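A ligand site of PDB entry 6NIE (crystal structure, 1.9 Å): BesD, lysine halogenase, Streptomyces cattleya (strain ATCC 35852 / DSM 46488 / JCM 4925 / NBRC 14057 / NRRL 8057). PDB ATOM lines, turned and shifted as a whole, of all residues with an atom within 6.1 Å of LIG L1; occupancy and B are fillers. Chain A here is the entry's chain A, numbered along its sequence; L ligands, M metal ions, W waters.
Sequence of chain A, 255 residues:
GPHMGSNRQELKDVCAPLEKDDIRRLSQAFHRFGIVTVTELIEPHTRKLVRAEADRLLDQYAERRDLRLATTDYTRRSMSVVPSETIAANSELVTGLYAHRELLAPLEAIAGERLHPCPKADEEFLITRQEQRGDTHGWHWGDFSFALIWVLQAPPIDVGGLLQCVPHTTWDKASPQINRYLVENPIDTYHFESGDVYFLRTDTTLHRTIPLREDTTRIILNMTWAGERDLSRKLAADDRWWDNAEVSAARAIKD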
ATOM      1  N   LEU A  69      32.326   6.419 -14.512  1.00  0.00           N
ATOM      2  CA  LEU A  69      31.430   5.449 -13.893  1.00  0.00           C
ATOM      3  C   LEU A  69      30.357   5.010 -14.879  1.00  0.00           C
ATOM      4  O   LEU A  69      29.517   5.830 -15.298  1.00  0.00           O
ATOM      5  CB  LEU A  69      30.798   6.041 -12.629  1.00  0.00           C
ATOM      6  CG  LEU A  69      30.229   4.935 -11.771  1.00  0.00           C
ATOM      7  CD1 LEU A  69      31.391   4.103 -11.265  1.00  0.00           C
ATOM      8  CD2 LEU A  69      29.467   5.505 -10.650  1.00  0.00           C
ATOM      9  N   THR A  72      26.638   5.897 -14.333  1.00  0.00           N
ATOM     10  CA  THR A  72      26.172   7.267 -14.532  1.00  0.00           C
ATOM     11  C   THR A  72      26.665   7.824 -15.874  1.00  0.00           C
ATOM     12  O   THR A  72      27.251   8.905 -15.907  1.00  0.00           O
ATOM     13  CB  THR A  72      26.596   8.223 -13.374  1.00  0.00           C
ATOM     14  OG1 THR A  72      28.016   8.356 -13.303  1.00  0.00           O
ATOM     15  CG2 THR A  72      26.067   7.791 -12.013  1.00  0.00           C
ATOM     16  N   ARG A  77      34.751  11.005 -12.036  1.00  0.00           N
ATOM     17  CA  ARG A  77      35.063  11.229 -10.633  1.00  0.00           C
ATOM     18  C   ARG A  77      36.559  11.485 -10.595  1.00  0.00           C
ATOM     19  O   ARG A  77      37.359  10.581 -10.868  1.00  0.00           O
ATOM     20  CB  ARG A  77      34.704  10.009  -9.787  1.00  0.00           C
ATOM     21  CG  ARG A  77      33.258   9.559  -9.933  1.00  0.00           C
ATOM     22  CD  ARG A  77      32.231  10.610  -9.415  1.00  0.00           C
ATOM     23  NE  ARG A  77      30.909   9.981  -9.504  1.00  0.00           N
ATOM     24  CZ  ARG A  77      30.236   9.813 -10.631  1.00  0.00           C
ATOM     25  NH1 ARG A  77      30.691  10.315 -11.782  1.00  0.00           N
ATOM     26  NH2 ARG A  77      29.075   9.181 -10.612  1.00  0.00           N
ATOM     27  N   GLU A 123      29.269   3.361   3.035  1.00  0.00           N
ATOM     28  CA  GLU A 123      28.722   4.629   2.566  1.00  0.00           C
ATOM     29  C   GLU A 123      28.092   5.466   3.683  1.00  0.00           C
ATOM     30  O   GLU A 123      27.359   6.420   3.392  1.00  0.00           O
ATOM     31  CB  GLU A 123      27.672   4.396   1.465  1.00  0.00           C
ATOM     32  CG  GLU A 123      27.352   5.690   0.740  1.00  0.00           C
ATOM     33  CD  GLU A 123      26.410   5.520  -0.435  1.00  0.00           C
ATOM     34  OE1 GLU A 123      26.017   4.370  -0.760  1.00  0.00           O
ATOM     35  OE2 GLU A 123      26.058   6.566  -1.019  1.00  0.00           O
ATOM     36  N   PHE A 125      29.908   7.492   5.579  1.00  0.00           N
ATOM     37  CA  PHE A 125      30.660   8.721   5.515  1.00  0.00           C
ATOM     38  C   PHE A 125      31.503   8.735   4.263  1.00  0.00           C
ATOM     39  O   PHE A 125      31.956   7.691   3.803  1.00  0.00           O
ATOM     40  CB  PHE A 125      31.586   8.854   6.721  1.00  0.00           C
ATOM     41  CG  PHE A 125      30.922   8.584   8.020  1.00  0.00           C
ATOM     42  CD1 PHE A 125      29.918   9.421   8.472  1.00  0.00           C
ATOM     43  CD2 PHE A 125      31.277   7.487   8.774  1.00  0.00           C
ATOM     44  CE1 PHE A 125      29.293   9.176   9.657  1.00  0.00           C
ATOM     45  CE2 PHE A 125      30.639   7.217   9.984  1.00  0.00           C
ATOM     46  CZ  PHE A 125      29.657   8.053  10.430  1.00  0.00           C
ATOM     47  N   LEU A 126      31.751   9.935   3.738  1.00  0.00           N
ATOM     48  CA  LEU A 126      32.754  10.091   2.700  1.00  0.00           C
ATOM     49  C   LEU A 126      33.338  11.488   2.807  1.00  0.00           C
ATOM     50  O   LEU A 126      32.586  12.462   2.895  1.00  0.00           O
ATOM     51  CB  LEU A 126      32.164   9.868   1.299  1.00  0.00           C
ATOM     52  CG  LEU A 126      33.077  10.021   0.059  1.00  0.00           C
ATOM     53  CD1 LEU A 126      34.107   8.911   0.058  1.00  0.00           C
ATOM     54  CD2 LEU A 126      32.273  10.001  -1.175  1.00  0.00           C
ATOM     55  N   HIS A 137      33.068  16.199  -9.302  1.00  0.00           N
ATOM     56  CA  HIS A 137      32.219  15.079  -8.906  1.00  0.00           C
ATOM     57  C   HIS A 137      31.105  15.043  -9.952  1.00  0.00           C
ATOM     58  O   HIS A 137      30.119  15.784  -9.850  1.00  0.00           O
ATOM     59  CB  HIS A 137      31.706  15.272  -7.472  1.00  0.00           C
ATOM     60  CG  HIS A 137      31.231  14.006  -6.832  1.00  0.00           C
ATOM     61  ND1 HIS A 137      31.334  13.777  -5.474  1.00  0.00           N
ATOM     62  CD2 HIS A 137      30.658  12.895  -7.358  1.00  0.00           C
ATOM     63  CE1 HIS A 137      30.834  12.583  -5.198  1.00  0.00           C
ATOM     64  NE2 HIS A 137      30.395  12.039  -6.312  1.00  0.00           N
ATOM     65  N   GLY A 138      31.275  14.208 -10.985  1.00  0.00           N
ATOM     66  CA  GLY A 138      30.439  14.286 -12.168  1.00  0.00           C
ATOM     67  C   GLY A 138      29.010  13.873 -11.911  1.00  0.00           C
ATOM     68  O   GLY A 138      28.657  13.353 -10.854  1.00  0.00           O
ATOM     69  N   TRP A 139      28.153  14.121 -12.912  1.00  0.00           N
ATOM     70  CA  TRP A 139      26.717  13.932 -12.682  1.00  0.00           C
ATOM     71  C   TRP A 139      26.414  12.546 -12.141  1.00  0.00           C
ATOM     72  O   TRP A 139      26.914  11.551 -12.657  1.00  0.00           O
ATOM     73  CB  TRP A 139      25.933  14.128 -13.977  1.00  0.00           C
ATOM     74  CG  TRP A 139      25.762  15.534 -14.455  1.00  0.00           C
ATOM     75  CD1 TRP A 139      26.319  16.090 -15.568  1.00  0.00           C
ATOM     76  CD2 TRP A 139      24.933  16.557 -13.874  1.00  0.00           C
ATOM     77  NE1 TRP A 139      25.883  17.387 -15.733  1.00  0.00           N
ATOM     78  CE2 TRP A 139      25.032  17.706 -14.705  1.00  0.00           C
ATOM     79  CE3 TRP A 139      24.110  16.618 -12.727  1.00  0.00           C
ATOM     80  CZ2 TRP A 139      24.360  18.894 -14.437  1.00  0.00           C
ATOM     81  CZ3 TRP A 139      23.429  17.846 -12.445  1.00  0.00           C
ATOM     82  CH2 TRP A 139      23.570  18.961 -13.306  1.00  0.00           C
ATOM     83  N   HIS A 140      25.507  12.482 -11.158  1.00  0.00           N
ATOM     84  CA  HIS A 140      25.142  11.220 -10.509  1.00  0.00           C
ATOM     85  C   HIS A 140      23.957  11.421  -9.577  1.00  0.00           C
ATOM     86  O   HIS A 140      23.537  12.544  -9.293  1.00  0.00           O
ATOM     87  CB  HIS A 140      26.308  10.658  -9.714  1.00  0.00           C
ATOM     88  CG  HIS A 140      26.669  11.515  -8.548  1.00  0.00           C
ATOM     89  ND1 HIS A 140      27.523  12.598  -8.672  1.00  0.00           N
ATOM     90  CD2 HIS A 140      26.328  11.455  -7.240  1.00  0.00           C
ATOM     91  CE1 HIS A 140      27.640  13.194  -7.505  1.00  0.00           C
ATOM     92  NE2 HIS A 140      26.969  12.490  -6.609  1.00  0.00           N
ATOM     93  N   TRP A 141      23.426  10.307  -9.096  1.00  0.00           N
ATOM     94  CA  TRP A 141      22.491  10.240  -7.979  1.00  0.00           C
ATOM     95  C   TRP A 141      23.117   9.416  -6.850  1.00  0.00           C
ATOM     96  O   TRP A 141      24.200   8.852  -6.996  1.00  0.00           O
ATOM     97  CB  TRP A 141      21.177   9.569  -8.399  1.00  0.00           C
ATOM     98  CG  TRP A 141      20.371  10.232  -9.464  1.00  0.00           C
ATOM     99  CD1 TRP A 141      19.305  11.043  -9.280  1.00  0.00           C
ATOM    100  CD2 TRP A 141      20.530  10.080 -10.890  1.00  0.00           C
ATOM    101  NE1 TRP A 141      18.770  11.406 -10.476  1.00  0.00           N
ATOM    102  CE2 TRP A 141      19.512  10.852 -11.489  1.00  0.00           C
ATOM    103  CE3 TRP A 141      21.431   9.390 -11.715  1.00  0.00           C
ATOM    104  CZ2 TRP A 141      19.341  10.922 -12.882  1.00  0.00           C
ATOM    105  CZ3 TRP A 141      21.275   9.481 -13.124  1.00  0.00           C
ATOM    106  CH2 TRP A 141      20.232  10.256 -13.680  1.00  0.00           C
ATOM    107  N   GLY A 142      22.398   9.316  -5.725  1.00  0.00           N
ATOM    108  CA  GLY A 142      22.759   8.451  -4.621  1.00  0.00           C
ATOM    109  C   GLY A 142      21.918   7.199  -4.558  1.00  0.00           C
ATOM    110  O   GLY A 142      20.758   7.186  -4.959  1.00  0.00           O
ATOM    111  N   ASP A 143      22.534   6.120  -4.037  1.00  0.00           N
ATOM    112  CA  ASP A 143      21.794   4.924  -3.689  1.00  0.00           C
ATOM    113  C   ASP A 143      20.794   5.181  -2.574  1.00  0.00           C
ATOM    114  O   ASP A 143      19.715   4.554  -2.526  1.00  0.00           O
ATOM    115  CB  ASP A 143      22.789   3.818  -3.304  1.00  0.00           C
ATOM    116  CG  ASP A 143      23.680   3.407  -4.487  1.00  0.00           C
ATOM    117  OD1 ASP A 143      23.134   2.875  -5.484  1.00  0.00           O
ATOM    118  OD2 ASP A 143      24.921   3.658  -4.445  1.00  0.00           O
ATOM    119  N   ALA A 147      21.709  12.992   2.216  1.00  0.00           N
ATOM    120  CA  ALA A 147      23.086  13.298   2.582  1.00  0.00           C
ATOM    121  C   ALA A 147      23.121  14.680   3.221  1.00  0.00           C
ATOM    122  O   ALA A 147      22.446  15.611   2.762  1.00  0.00           O
ATOM    123  CB  ALA A 147      24.041  13.237   1.377  1.00  0.00           C
ATOM    124  N   TRP A 171      17.287   7.543 -10.639  1.00  0.00           N
ATOM    125  CA  TRP A 171      18.498   6.896 -11.110  1.00  0.00           C
ATOM    126  C   TRP A 171      18.136   5.513 -11.607  1.00  0.00           C
ATOM    127  O   TRP A 171      17.846   4.618 -10.797  1.00  0.00           O
ATOM    128  CB  TRP A 171      19.523   6.802  -9.984  1.00  0.00           C
ATOM    129  CG  TRP A 171      20.861   6.348 -10.463  1.00  0.00           C
ATOM    130  CD1 TRP A 171      21.258   6.176 -11.785  1.00  0.00           C
ATOM    131  CD2 TRP A 171      21.997   6.037  -9.651  1.00  0.00           C
ATOM    132  NE1 TRP A 171      22.567   5.764 -11.812  1.00  0.00           N
ATOM    133  CE2 TRP A 171      23.054   5.664 -10.528  1.00  0.00           C
ATOM    134  CE3 TRP A 171      22.227   6.024  -8.253  1.00  0.00           C
ATOM    135  CZ2 TRP A 171      24.321   5.304 -10.069  1.00  0.00           C
ATOM    136  CZ3 TRP A 171      23.480   5.660  -7.793  1.00  0.00           C
ATOM    137  CH2 TRP A 171      24.526   5.311  -8.712  1.00  0.00           C
ATOM    138  N   ASN A 222      30.555  14.061   3.694  1.00  0.00           N
ATOM    139  CA  ASN A 222      29.223  13.565   3.364  1.00  0.00           C
ATOM    140  C   ASN A 222      28.848  12.558   4.450  1.00  0.00           C
ATOM    141  O   ASN A 222      29.587  11.590   4.696  1.00  0.00           O
ATOM    142  CB  ASN A 222      29.226  12.934   1.971  1.00  0.00           C
ATOM    143  CG  ASN A 222      27.896  12.307   1.569  1.00  0.00           C
ATOM    144  OD1 ASN A 222      27.167  11.774   2.398  1.00  0.00           O
ATOM    145  ND2 ASN A 222      27.612  12.314   0.263  1.00  0.00           N
ATOM    146  N   THR A 224      25.663  10.085   5.014  1.00  0.00           N
ATOM    147  CA  THR A 224      24.531   9.554   4.262  1.00  0.00           C
ATOM    148  C   THR A 224      23.637   8.707   5.148  1.00  0.00           C
ATOM    149  O   THR A 224      24.136   7.849   5.880  1.00  0.00           O
ATOM    150  CB  THR A 224      25.020   8.739   3.052  1.00  0.00           C
ATOM    151  OG1 THR A 224      25.396   9.642   2.002  1.00  0.00           O
ATOM    152  CG2 THR A 224      23.909   7.819   2.536  1.00  0.00           C
ATOM    153  N   ASP A 239      29.410  -0.663  -8.648  1.00  0.00           N
ATOM    154  CA  ASP A 239      29.767   0.702  -9.027  1.00  0.00           C
ATOM    155  C   ASP A 239      30.210   1.557  -7.848  1.00  0.00           C
ATOM    156  O   ASP A 239      30.202   2.785  -7.951  1.00  0.00           O
ATOM    157  CB  ASP A 239      28.618   1.399  -9.763  1.00  0.00           C
ATOM    158  CG  ASP A 239      27.393   1.629  -8.864  1.00  0.00           C
ATOM    159  OD1 ASP A 239      27.364   1.078  -7.743  1.00  0.00           O
ATOM    160  OD2 ASP A 239      26.461   2.348  -9.280  1.00  0.00           O
ATOM    161  N   TRP A 241      32.653   3.056  -6.405  1.00  0.00           N
ATOM    162  CA  TRP A 241      34.004   3.464  -6.773  1.00  0.00           C
ATOM    163  C   TRP A 241      34.740   4.189  -5.624  1.00  0.00           C
ATOM    164  O   TRP A 241      35.973   4.145  -5.579  1.00  0.00           O
ATOM    165  CB  TRP A 241      33.925   4.397  -8.006  1.00  0.00           C
ATOM    166  CG  TRP A 241      33.103   5.623  -7.678  1.00  0.00           C
ATOM    167  CD1 TRP A 241      31.742   5.775  -7.830  1.00  0.00           C
ATOM    168  CD2 TRP A 241      33.569   6.843  -7.088  1.00  0.00           C
ATOM    169  NE1 TRP A 241      31.357   7.009  -7.387  1.00  0.00           N
ATOM    170  CE2 TRP A 241      32.447   7.691  -6.927  1.00  0.00           C
ATOM    171  CE3 TRP A 241      34.825   7.301  -6.677  1.00  0.00           C
ATOM    172  CZ2 TRP A 241      32.540   8.959  -6.343  1.00  0.00           C
ATOM    173  CZ3 TRP A 241      34.922   8.574  -6.115  1.00  0.00           C
ATOM    174  CH2 TRP A 241      33.787   9.382  -5.961  1.00  0.00           C
ATOM    175  N   TRP A 242      34.013   4.886  -4.747  1.00  0.00           N
ATOM    176  CA  TRP A 242      34.686   5.687  -3.715  1.00  0.00           C
ATOM    177  C   TRP A 242      35.363   4.777  -2.706  1.00  0.00           C
ATOM    178  O   TRP A 242      36.399   5.144  -2.125  1.00  0.00           O
ATOM    179  CB  TRP A 242      33.694   6.631  -3.008  1.00  0.00           C
ATOM    180  CG  TRP A 242      32.581   5.892  -2.322  1.00  0.00           C
ATOM    181  CD1 TRP A 242      32.534   5.485  -0.988  1.00  0.00           C
ATOM    182  CD2 TRP A 242      31.384   5.396  -2.932  1.00  0.00           C
ATOM    183  NE1 TRP A 242      31.366   4.808  -0.758  1.00  0.00           N
ATOM    184  CE2 TRP A 242      30.645   4.726  -1.918  1.00  0.00           C
ATOM    185  CE3 TRP A 242      30.850   5.471  -4.230  1.00  0.00           C
ATOM    186  CZ2 TRP A 242      29.408   4.118  -2.170  1.00  0.00           C
ATOM    187  CZ3 TRP A 242      29.611   4.875  -4.475  1.00  0.00           C
ATOM    188  CH2 TRP A 242      28.912   4.198  -3.451  1.00  0.00           C
HETATM  189  N1  LIG L   1      26.561   7.715  -5.867  1.00  0.00           N
HETATM  190  C1  LIG L   1      27.681   8.655  -5.717  1.00  0.00           C
HETATM  191  C2  LIG L   1      28.490   8.789  -7.011  1.00  0.00           C
HETATM  192  O1  LIG L   1      29.444   9.594  -7.115  1.00  0.00           O
HETATM  193  C3  LIG L   1      28.599   8.238  -4.555  1.00  0.00           C
HETATM  194  C4  LIG L   1      28.086   8.686  -3.144  1.00  0.00           C
HETATM  195  C5  LIG L   1      29.037   8.179  -2.018  1.00  0.00           C
HETATM  196  C6  LIG L   1      28.770   8.878  -0.660  1.00  0.00           C
HETATM  197  N2  LIG L   1      27.345   8.652  -0.172  1.00  0.00           N
HETATM  198  O2  LIG L   1      28.199   8.126  -7.994  1.00  0.00           O
HETATM  199  C1  LG2 L   2      28.356  13.467  -2.641  1.00  0.00           C
HETATM  200  O1  LG2 L   2      27.654  12.485  -2.934  1.00  0.00           O
HETATM  201  O2  LG2 L   2      29.123  13.547  -1.646  1.00  0.00           O
HETATM  202  C2  LG2 L   2      28.329  14.619  -3.543  1.00  0.00           C
HETATM  203  O3  LG2 L   2      27.627  14.611  -4.515  1.00  0.00           O
HETATM  204  C3  LG2 L   2      29.267  15.731  -3.204  1.00  0.00           C
HETATM  205  C4  LG2 L   2      28.657  17.057  -3.051  1.00  0.00           C
HETATM  206  C5  LG2 L   2      29.710  18.195  -2.986  1.00  0.00           C
HETATM  207  O4  LG2 L   2      29.325  19.325  -2.577  1.00  0.00           O
HETATM  208  O5  LG2 L   2      30.903  17.955  -3.320  1.00  0.00           O
HETATM  209 FE    FE M   1      26.249  12.916  -4.524  1.00  0.00          FE
HETATM  210  O   HOH W   1      25.588   6.037  -3.698  1.00  0.00           O
HETATM  211  O   HOH W   2      28.538   9.007   2.494  1.00  0.00           O
HETATM  212  O   HOH W   3      27.780   5.334  -7.100  1.00  0.00           O
HETATM  213  O   HOH W   4      25.588  10.625  -1.018  1.00  0.00           O
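OE2 of Glu 123 is in salt-bridge range of N2 of LIG L1 (2.6 Å).
A ring nitrogen (NE2) of His 137 sits at hydrogen-bond distance from an oxygen (O1) of LIG L1, 2.7 Å away.
The guanidinium group of Arg 77 lies within salt-bridge range of an oxygen (O1) of LIG L1 (2.8 Å).
The backbone carbonyl oxygen (O) of Trp 141 lies within hydrogen-bond range of a nitrogen (N1) of LIG L1 (2.9 Å).
OG1 of Thr 224 lies within hydrogen-bond range of N2 of LIG L1 (3.1 Å).
The indole nitrogen (NE1) of Trp 241 is in hydrogen-bond range of an oxygen (O1) of LIG L1 (3.2 Å).
The side-chain amide nitrogen of Asn 222 is in hydrogen-bond range of an oxygen (O2) of LG2 L2.
A ring nitrogen (NE2) of His 140 sits close to a ring nitrogen (NE2) of His 137 (3.5 Å).
The side-chain hydroxyl (OG1) of Thr 72 is in hydrogen-bond range of the guanidinium group (NH2) of Arg 77, at 3.0 Å.
The side-chain amide oxygen (OD1) of Asn 222 is in hydrogen-bond range of the side-chain hydroxyl (OG1) of Thr 224, at 2.8 Å.
The backbone carbonyl oxygen (O) of Gly 138 sits at hydrogen-bond distance from a ring nitrogen (ND1) of His 140, 2.6 Å away.
The backbone carbonyl oxygen (O) of Leu 126 is in hydrogen-bond range of the backbone NH (N) of Asn 222 (2.7 Å).
Leu 69 touches LIG L1.
CD2 of Leu 126 touches C6 of LIG L1, at 3.7 Å.
CD2 of His 140 touches C2 of LIG L1, 3.4 Å away.
ND2 of Asn 222 touches N2 of LIG L1 (3.7 Å).
CZ3 of Trp 242 touches C3 of LIG L1, at 3.5 Å.
Hydrophobic or aromatic side chains within 4 Å of LIG L1: Leu 69, Leu 126, His 137, His 140, Trp 241 and Trp 242.
11 residues have an atom within 4 Å of LIG L1: Leu 69, Arg 77, Glu 123, Leu 126, His 137, His 140, Trp 141, Asn 222, Thr 224, Trp 241 and Trp 242.
Water W4 lies within hydrogen-bond range of N2 of LIG L1 (2.8 Å), ND2 of Asn 222 (2.9 Å) and OG1 of Thr 224 (3.2 Å).
Water W1 lies within hydrogen-bond range of OD2 of Asp 143, OE2 of Glu 123 and N1 of LIG L1.
Water W2 lies within hydrogen-bond range of N2 of LIG L1 (2.9 Å), O of Glu 123 (3.0 Å), OD1 of Asn 222 (3.1 Å) and OG1 of Thr 224 (3.2 Å).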
